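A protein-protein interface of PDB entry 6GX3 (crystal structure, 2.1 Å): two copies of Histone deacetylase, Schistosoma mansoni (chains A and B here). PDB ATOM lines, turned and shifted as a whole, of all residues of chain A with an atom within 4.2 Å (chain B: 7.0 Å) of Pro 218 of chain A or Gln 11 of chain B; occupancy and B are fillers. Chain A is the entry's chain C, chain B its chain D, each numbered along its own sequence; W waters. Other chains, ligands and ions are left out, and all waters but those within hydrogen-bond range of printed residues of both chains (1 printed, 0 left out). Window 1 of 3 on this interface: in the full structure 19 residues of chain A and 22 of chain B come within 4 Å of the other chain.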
ATOM      1  N   HIS A 190      19.761   8.548  15.111  1.00  0.00           N
ATOM      2  CA  HIS A 190      21.156   8.364  14.706  1.00  0.00           C
ATOM      3  C   HIS A 190      21.405   6.971  14.121  1.00  0.00           C
ATOM      4  O   HIS A 190      21.076   5.966  14.754  1.00  0.00           O
ATOM      5  CB  HIS A 190      22.100   8.568  15.886  1.00  0.00           C
ATOM      6  CG  HIS A 190      23.539   8.371  15.529  1.00  0.00           C
ATOM      7  ND1 HIS A 190      24.417   7.655  16.316  1.00  0.00           N
ATOM      8  CD2 HIS A 190      24.253   8.800  14.458  1.00  0.00           C
ATOM      9  CE1 HIS A 190      25.609   7.650  15.745  1.00  0.00           C
ATOM     10  NE2 HIS A 190      25.539   8.333  14.615  1.00  0.00           N
ATOM     11  N   ASP A 192      23.490   4.644  14.186  1.00  0.00           N
ATOM     12  CA  ASP A 192      24.674   4.216  14.945  1.00  0.00           C
ATOM     13  C   ASP A 192      25.304   2.912  14.455  1.00  0.00           C
ATOM     14  O   ASP A 192      26.537   2.761  14.472  1.00  0.00           O
ATOM     15  CB  ASP A 192      24.322   4.079  16.431  1.00  0.00           C
ATOM     16  CG  ASP A 192      23.137   3.126  16.687  1.00  0.00           C
ATOM     17  OD1 ASP A 192      22.377   2.801  15.745  1.00  0.00           O
ATOM     18  OD2 ASP A 192      22.960   2.712  17.851  1.00  0.00           O
ATOM     19  N   PHE A 216      17.232  10.109  24.707  1.00  0.00           N
ATOM     20  CA  PHE A 216      16.619   9.724  23.428  1.00  0.00           C
ATOM     21  C   PHE A 216      17.471   8.690  22.685  1.00  0.00           C
ATOM     22  O   PHE A 216      18.657   8.889  22.472  1.00  0.00           O
ATOM     23  CB  PHE A 216      16.394  10.965  22.552  1.00  0.00           C
ATOM     24  CG  PHE A 216      15.704  10.678  21.240  1.00  0.00           C
ATOM     25  CD1 PHE A 216      14.355  10.394  21.195  1.00  0.00           C
ATOM     26  CD2 PHE A 216      16.407  10.749  20.049  1.00  0.00           C
ATOM     27  CE1 PHE A 216      13.726  10.140  19.987  1.00  0.00           C
ATOM     28  CE2 PHE A 216      15.794  10.492  18.850  1.00  0.00           C
ATOM     29  CZ  PHE A 216      14.448  10.193  18.810  1.00  0.00           C
ATOM     30  N   PHE A 217      16.838   7.590  22.285  1.00  0.00           N
ATOM     31  CA  PHE A 217      17.479   6.487  21.561  1.00  0.00           C
ATOM     32  C   PHE A 217      18.170   6.902  20.262  1.00  0.00           C
ATOM     33  O   PHE A 217      17.632   7.696  19.508  1.00  0.00           O
ATOM     34  CB  PHE A 217      16.416   5.426  21.243  1.00  0.00           C
ATOM     35  CG  PHE A 217      16.969   4.167  20.671  1.00  0.00           C
ATOM     36  CD1 PHE A 217      17.130   4.021  19.306  1.00  0.00           C
ATOM     37  CD2 PHE A 217      17.330   3.125  21.501  1.00  0.00           C
ATOM     38  CE1 PHE A 217      17.637   2.868  18.778  1.00  0.00           C
ATOM     39  CE2 PHE A 217      17.839   1.962  20.976  1.00  0.00           C
ATOM     40  CZ  PHE A 217      17.992   1.835  19.611  1.00  0.00           C
ATOM     41  N   PRO A 218      19.364   6.351  19.978  1.00  0.00           N
ATOM     42  CA  PRO A 218      20.150   5.416  20.788  1.00  0.00           C
ATOM     43  C   PRO A 218      21.178   6.123  21.688  1.00  0.00           C
ATOM     44  O   PRO A 218      21.876   5.452  22.438  1.00  0.00           O
ATOM     45  CB  PRO A 218      20.834   4.550  19.733  1.00  0.00           C
ATOM     46  CG  PRO A 218      21.112   5.549  18.616  1.00  0.00           C
ATOM     47  CD  PRO A 218      19.949   6.534  18.636  1.00  0.00           C
ATOM     48  N   GLY A 219      21.253   7.452  21.623  1.00  0.00           N
ATOM     49  CA  GLY A 219      22.078   8.229  22.536  1.00  0.00           C
ATOM     50  C   GLY A 219      23.288   8.878  21.880  1.00  0.00           C
ATOM     51  O   GLY A 219      23.795   9.890  22.358  1.00  0.00           O
ATOM     52  N   THR A 220      23.739   8.291  20.776  1.00  0.00           N
ATOM     53  CA  THR A 220      24.918   8.740  20.054  1.00  0.00           C
ATOM     54  C   THR A 220      24.586   9.756  18.970  1.00  0.00           C
ATOM     55  O   THR A 220      23.428  10.116  18.790  1.00  0.00           O
ATOM     56  CB  THR A 220      25.628   7.562  19.391  1.00  0.00           C
ATOM     57  OG1 THR A 220      24.655   6.751  18.719  1.00  0.00           O
ATOM     58  CG2 THR A 220      26.391   6.721  20.430  1.00  0.00           C
ATOM     59  N   TYR B   8      23.924  -2.868  32.495  1.00  0.00           N
ATOM     60  CA  TYR B   8      25.130  -2.291  31.900  1.00  0.00           C
ATOM     61  C   TYR B   8      24.998  -2.013  30.410  1.00  0.00           C
ATOM     62  O   TYR B   8      24.005  -2.373  29.773  1.00  0.00           O
ATOM     63  CB  TYR B   8      26.365  -3.168  32.159  1.00  0.00           C
ATOM     64  CG  TYR B   8      26.403  -4.525  31.502  1.00  0.00           C
ATOM     65  CD1 TYR B   8      26.952  -4.694  30.231  1.00  0.00           C
ATOM     66  CD2 TYR B   8      25.939  -5.652  32.172  1.00  0.00           C
ATOM     67  CE1 TYR B   8      27.002  -5.949  29.634  1.00  0.00           C
ATOM     68  CE2 TYR B   8      25.988  -6.910  31.585  1.00  0.00           C
ATOM     69  CZ  TYR B   8      26.518  -7.053  30.318  1.00  0.00           C
ATOM     70  OH  TYR B   8      26.557  -8.306  29.746  1.00  0.00           O
ATOM     71  N   GLY B   9      26.015  -1.341  29.877  1.00  0.00           N
ATOM     72  CA  GLY B   9      26.038  -0.906  28.494  1.00  0.00           C
ATOM     73  C   GLY B   9      27.224   0.014  28.289  1.00  0.00           C
ATOM     74  O   GLY B   9      27.682   0.643  29.243  1.00  0.00           O
ATOM     75  N   ASP B  10      27.717   0.096  27.053  1.00  0.00           N
ATOM     76  CA  ASP B  10      28.946   0.836  26.757  1.00  0.00           C
ATOM     77  C   ASP B  10      28.792   2.319  27.039  1.00  0.00           C
ATOM     78  O   ASP B  10      29.664   2.941  27.653  1.00  0.00           O
ATOM     79  CB  ASP B  10      29.369   0.629  25.303  1.00  0.00           C
ATOM     80  CG  ASP B  10      29.956  -0.746  25.068  1.00  0.00           C
ATOM     81  OD1 ASP B  10      30.686  -1.235  25.960  1.00  0.00           O
ATOM     82  OD2 ASP B  10      29.683  -1.339  24.004  1.00  0.00           O
ATOM     83  N   GLN B  11      27.680   2.879  26.583  1.00  0.00           N
ATOM     84  CA  GLN B  11      27.385   4.270  26.850  1.00  0.00           C
ATOM     85  C   GLN B  11      27.116   4.458  28.340  1.00  0.00           C
ATOM     86  O   GLN B  11      27.536   5.453  28.931  1.00  0.00           O
ATOM     87  CB  GLN B  11      26.187   4.740  26.020  1.00  0.00           C
ATOM     88  CG  GLN B  11      26.498   4.974  24.559  1.00  0.00           C
ATOM     89  CD  GLN B  11      25.237   5.218  23.747  1.00  0.00           C
ATOM     90  OE1 GLN B  11      25.065   4.671  22.653  1.00  0.00           O
ATOM     91  NE2 GLN B  11      24.339   6.037  24.288  1.00  0.00           N
ATOM     92  N   TYR B  12      26.432   3.485  28.937  1.00  0.00           N
ATOM     93  CA  TYR B  12      26.024   3.565  30.334  1.00  0.00           C
ATOM     94  C   TYR B  12      27.264   3.681  31.191  1.00  0.00           C
ATOM     95  O   TYR B  12      27.348   4.512  32.104  1.00  0.00           O
ATOM     96  CB  TYR B  12      25.188   2.336  30.722  1.00  0.00           C
ATOM     97  CG  TYR B  12      24.608   2.378  32.114  1.00  0.00           C
ATOM     98  CD1 TYR B  12      23.587   3.269  32.434  1.00  0.00           C
ATOM     99  CD2 TYR B  12      25.056   1.507  33.101  1.00  0.00           C
ATOM    100  CE1 TYR B  12      23.043   3.301  33.703  1.00  0.00           C
ATOM    101  CE2 TYR B  12      24.516   1.528  34.376  1.00  0.00           C
ATOM    102  CZ  TYR B  12      23.506   2.436  34.667  1.00  0.00           C
ATOM    103  OH  TYR B  12      22.958   2.473  35.926  1.00  0.00           O
ATOM    104  N   ARG B  13      28.241   2.847  30.859  1.00  0.00           N
ATOM    105  CA  ARG B  13      29.527   2.838  31.535  1.00  0.00           C
ATOM    106  C   ARG B  13      30.239   4.191  31.408  1.00  0.00           C
ATOM    107  O   ARG B  13      30.781   4.716  32.377  1.00  0.00           O
ATOM    108  CB  ARG B  13      30.390   1.719  30.960  1.00  0.00           C
ATOM    109  CG  ARG B  13      31.737   1.544  31.608  1.00  0.00           C
ATOM    110  CD  ARG B  13      32.538   0.546  30.801  1.00  0.00           C
ATOM    111  NE  ARG B  13      33.922   0.508  31.238  1.00  0.00           N
ATOM    112  CZ  ARG B  13      34.537  -0.587  31.656  1.00  0.00           C
ATOM    113  NH1 ARG B  13      33.893  -1.743  31.671  1.00  0.00           N
ATOM    114  NH2 ARG B  13      35.804  -0.524  32.042  1.00  0.00           N
ATOM    115  N   GLN B  14      30.216   4.749  30.203  1.00  0.00           N
ATOM    116  CA  GLN B  14      30.851   6.031  29.920  1.00  0.00           C
ATOM    117  C   GLN B  14      30.212   7.148  30.749  1.00  0.00           C
ATOM    118  O   GLN B  14      30.907   7.981  31.335  1.00  0.00           O
ATOM    119  CB  GLN B  14      30.752   6.332  28.421  1.00  0.00           C
ATOM    120  CG  GLN B  14      31.657   7.435  27.909  1.00  0.00           C
ATOM    121  CD  GLN B  14      31.541   7.613  26.402  1.00  0.00           C
ATOM    122  OE1 GLN B  14      32.092   8.553  25.829  1.00  0.00           O
ATOM    123  NE2 GLN B  14      30.818   6.704  25.753  1.00  0.00           N
ATOM    124  N   LEU B  15      28.885   7.152  30.814  1.00  0.00           N
ATOM    125  CA  LEU B  15      28.165   8.158  31.597  1.00  0.00           C
ATOM    126  C   LEU B  15      28.394   8.014  33.111  1.00  0.00           C
ATOM    127  O   LEU B  15      28.706   8.994  33.794  1.00  0.00           O
ATOM    128  CB  LEU B  15      26.667   8.097  31.275  1.00  0.00           C
ATOM    129  CG  LEU B  15      26.319   8.737  29.929  1.00  0.00           C
ATOM    130  CD1 LEU B  15      24.878   8.466  29.521  1.00  0.00           C
ATOM    131  CD2 LEU B  15      26.607  10.226  29.977  1.00  0.00           C
ATOM    132  N   CYS B  16      28.254   6.801  33.638  1.00  0.00           N
ATOM    133  CA  CYS B  16      28.526   6.553  35.053  1.00  0.00           C
ATOM    134  C   CYS B  16      29.966   6.869  35.453  1.00  0.00           C
ATOM    135  O   CYS B  16      30.248   7.032  36.643  1.00  0.00           O
ATOM    136  CB  CYS B  16      28.214   5.095  35.421  1.00  0.00           C
ATOM    137  SG  CYS B  16      26.513   4.610  35.129  1.00  0.00           S
ATOM    138  N   CYS B  17      30.876   6.960  34.481  1.00  0.00           N
ATOM    139  CA  CYS B  17      32.262   7.332  34.784  1.00  0.00           C
ATOM    140  C   CYS B  17      32.602   8.779  34.393  1.00  0.00           C
ATOM    141  O   CYS B  17      33.772   9.126  34.264  1.00  0.00           O
ATOM    142  CB  CYS B  17      33.244   6.373  34.088  1.00  0.00           C
ATOM    143  SG  CYS B  17      33.083   4.626  34.575  1.00  0.00           S
ATOM    144  N   SER B  18      31.592   9.631  34.233  1.00  0.00           N
ATOM    145  CA  SER B  18      31.827  10.999  33.767  1.00  0.00           C
ATOM    146  C   SER B  18      31.847  12.042  34.891  1.00  0.00           C
ATOM    147  O   SER B  18      32.081  13.221  34.639  1.00  0.00           O
ATOM    148  CB  SER B  18      30.771  11.391  32.725  1.00  0.00           C
ATOM    149  OG  SER B  18      30.868  10.583  31.560  1.00  0.00           O
ATOM    150  N   PRO B  47      19.811  -0.060  29.946  1.00  0.00           N
ATOM    151  CA  PRO B  47      19.164   1.155  30.451  1.00  0.00           C
ATOM    152  C   PRO B  47      17.964   1.580  29.591  1.00  0.00           C
ATOM    153  O   PRO B  47      17.950   1.435  28.369  1.00  0.00           O
ATOM    154  CB  PRO B  47      20.275   2.201  30.381  1.00  0.00           C
ATOM    155  CG  PRO B  47      21.552   1.397  30.443  1.00  0.00           C
ATOM    156  CD  PRO B  47      21.254   0.131  29.702  1.00  0.00           C
ATOM    157  N   GLN B  49      15.498   3.844  27.534  1.00  0.00           N
ATOM    158  CA  GLN B  49      15.605   5.039  26.728  1.00  0.00           C
ATOM    159  C   GLN B  49      14.191   5.443  26.352  1.00  0.00           C
ATOM    160  O   GLN B  49      13.271   4.643  26.501  1.00  0.00           O
ATOM    161  CB  GLN B  49      16.499   4.799  25.516  1.00  0.00           C
ATOM    162  CG  GLN B  49      17.956   4.623  25.932  1.00  0.00           C
ATOM    163  CD  GLN B  49      18.881   4.379  24.772  1.00  0.00           C
ATOM    164  OE1 GLN B  49      18.990   3.263  24.280  1.00  0.00           O
ATOM    165  NE2 GLN B  49      19.561   5.425  24.330  1.00  0.00           N
ATOM    166  N   ALA B 114      21.401   8.895  33.447  1.00  0.00           N
ATOM    167  CA  ALA B 114      21.785   7.495  33.191  1.00  0.00           C
ATOM    168  C   ALA B 114      21.358   6.557  34.338  1.00  0.00           C
ATOM    169  O   ALA B 114      20.756   5.507  34.094  1.00  0.00           O
ATOM    170  CB  ALA B 114      23.285   7.399  32.949  1.00  0.00           C
HETATM  171  O   HOH W   1      24.582   3.994  19.745  1.00  0.00           O
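The backbone carbonyl oxygen of Pro 218 of chain A sits at hydrogen-bond distance from the side-chain amide nitrogen of Gln 11 of chain B, 3.1 Å away.
NE2 of Gln 49 of chain B lies within hydrogen-bond range of O of Pro 218 of chain A (3.0 Å).
The side-chain hydroxyl (OG1) of Thr 220 of chain A sits at hydrogen-bond distance from a ring nitrogen (ND1) of His 190 of chain A (2.6 Å).
Among the printed residues, merely in contact across the chains: Phe 217 of chain A with Gln 49 of chain B (3.2 Å), Gly 219 of chain A with Gln 11 of chain B (3.6 Å), Gly 219 of chain A with Gln 49 of chain B (3.8 Å) and Thr 220 of chain A with Gln 11 of chain B (3.3 Å).
Pro 218 of chain A touches just these residues of chain B: Gln 11 (3.1 Å) and Gln 49 (3.0 Å).
Of chain A, only Pro 218 (3.1 Å), Gly 219 (3.6 Å) and Thr 220 (3.3 Å) come within 4 Å of Gln 11 of chain B.
Printed residues of chain A within 4 Å of Gln 49 of chain B: Phe 217 (3.2 Å), Pro 218 (3.0 Å) and Gly 219 (3.8 Å).
Printed residues of chain B within 4 Å of Thr 220 of chain A: Gln 11 (3.3 Å).
Printed residues of chain B within 4 Å of Phe 217 of chain A: Gln 49.
Of the printed residues of chain B, Gly 219 of chain A touches Gln 11 and Gln 49.
The nearest printed residue of chain A that does not touch Gln 11 of chain B is Asp 192 of chain A (5.6 Å).
The nearest printed residue of chain B that does not touch Gly 219 of chain A is Leu 15 of chain B (7.4 Å).
Along chain B the printed residues that touch a printed residue of chain A span positions 11 to 49.
Among the printed residues, 6 pairs touch across the chains.
Among the printed residues, no Asp or Glu carboxylate lies within 4 Å of a Lys or Arg side-chain nitrogen of the other chain.
No position is printed for both chains.
Of the 6 pairs that touch across the chains among the printed residues, none has its exchanged pair printed and touching as well.
Water W1 lies within hydrogen-bond range of OD2 of Asp 192 of chain A (2.8 Å), OG1 of Thr 220 of chain A (2.9 Å) and OE1 of Gln 11 of chain B (3.0 Å).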
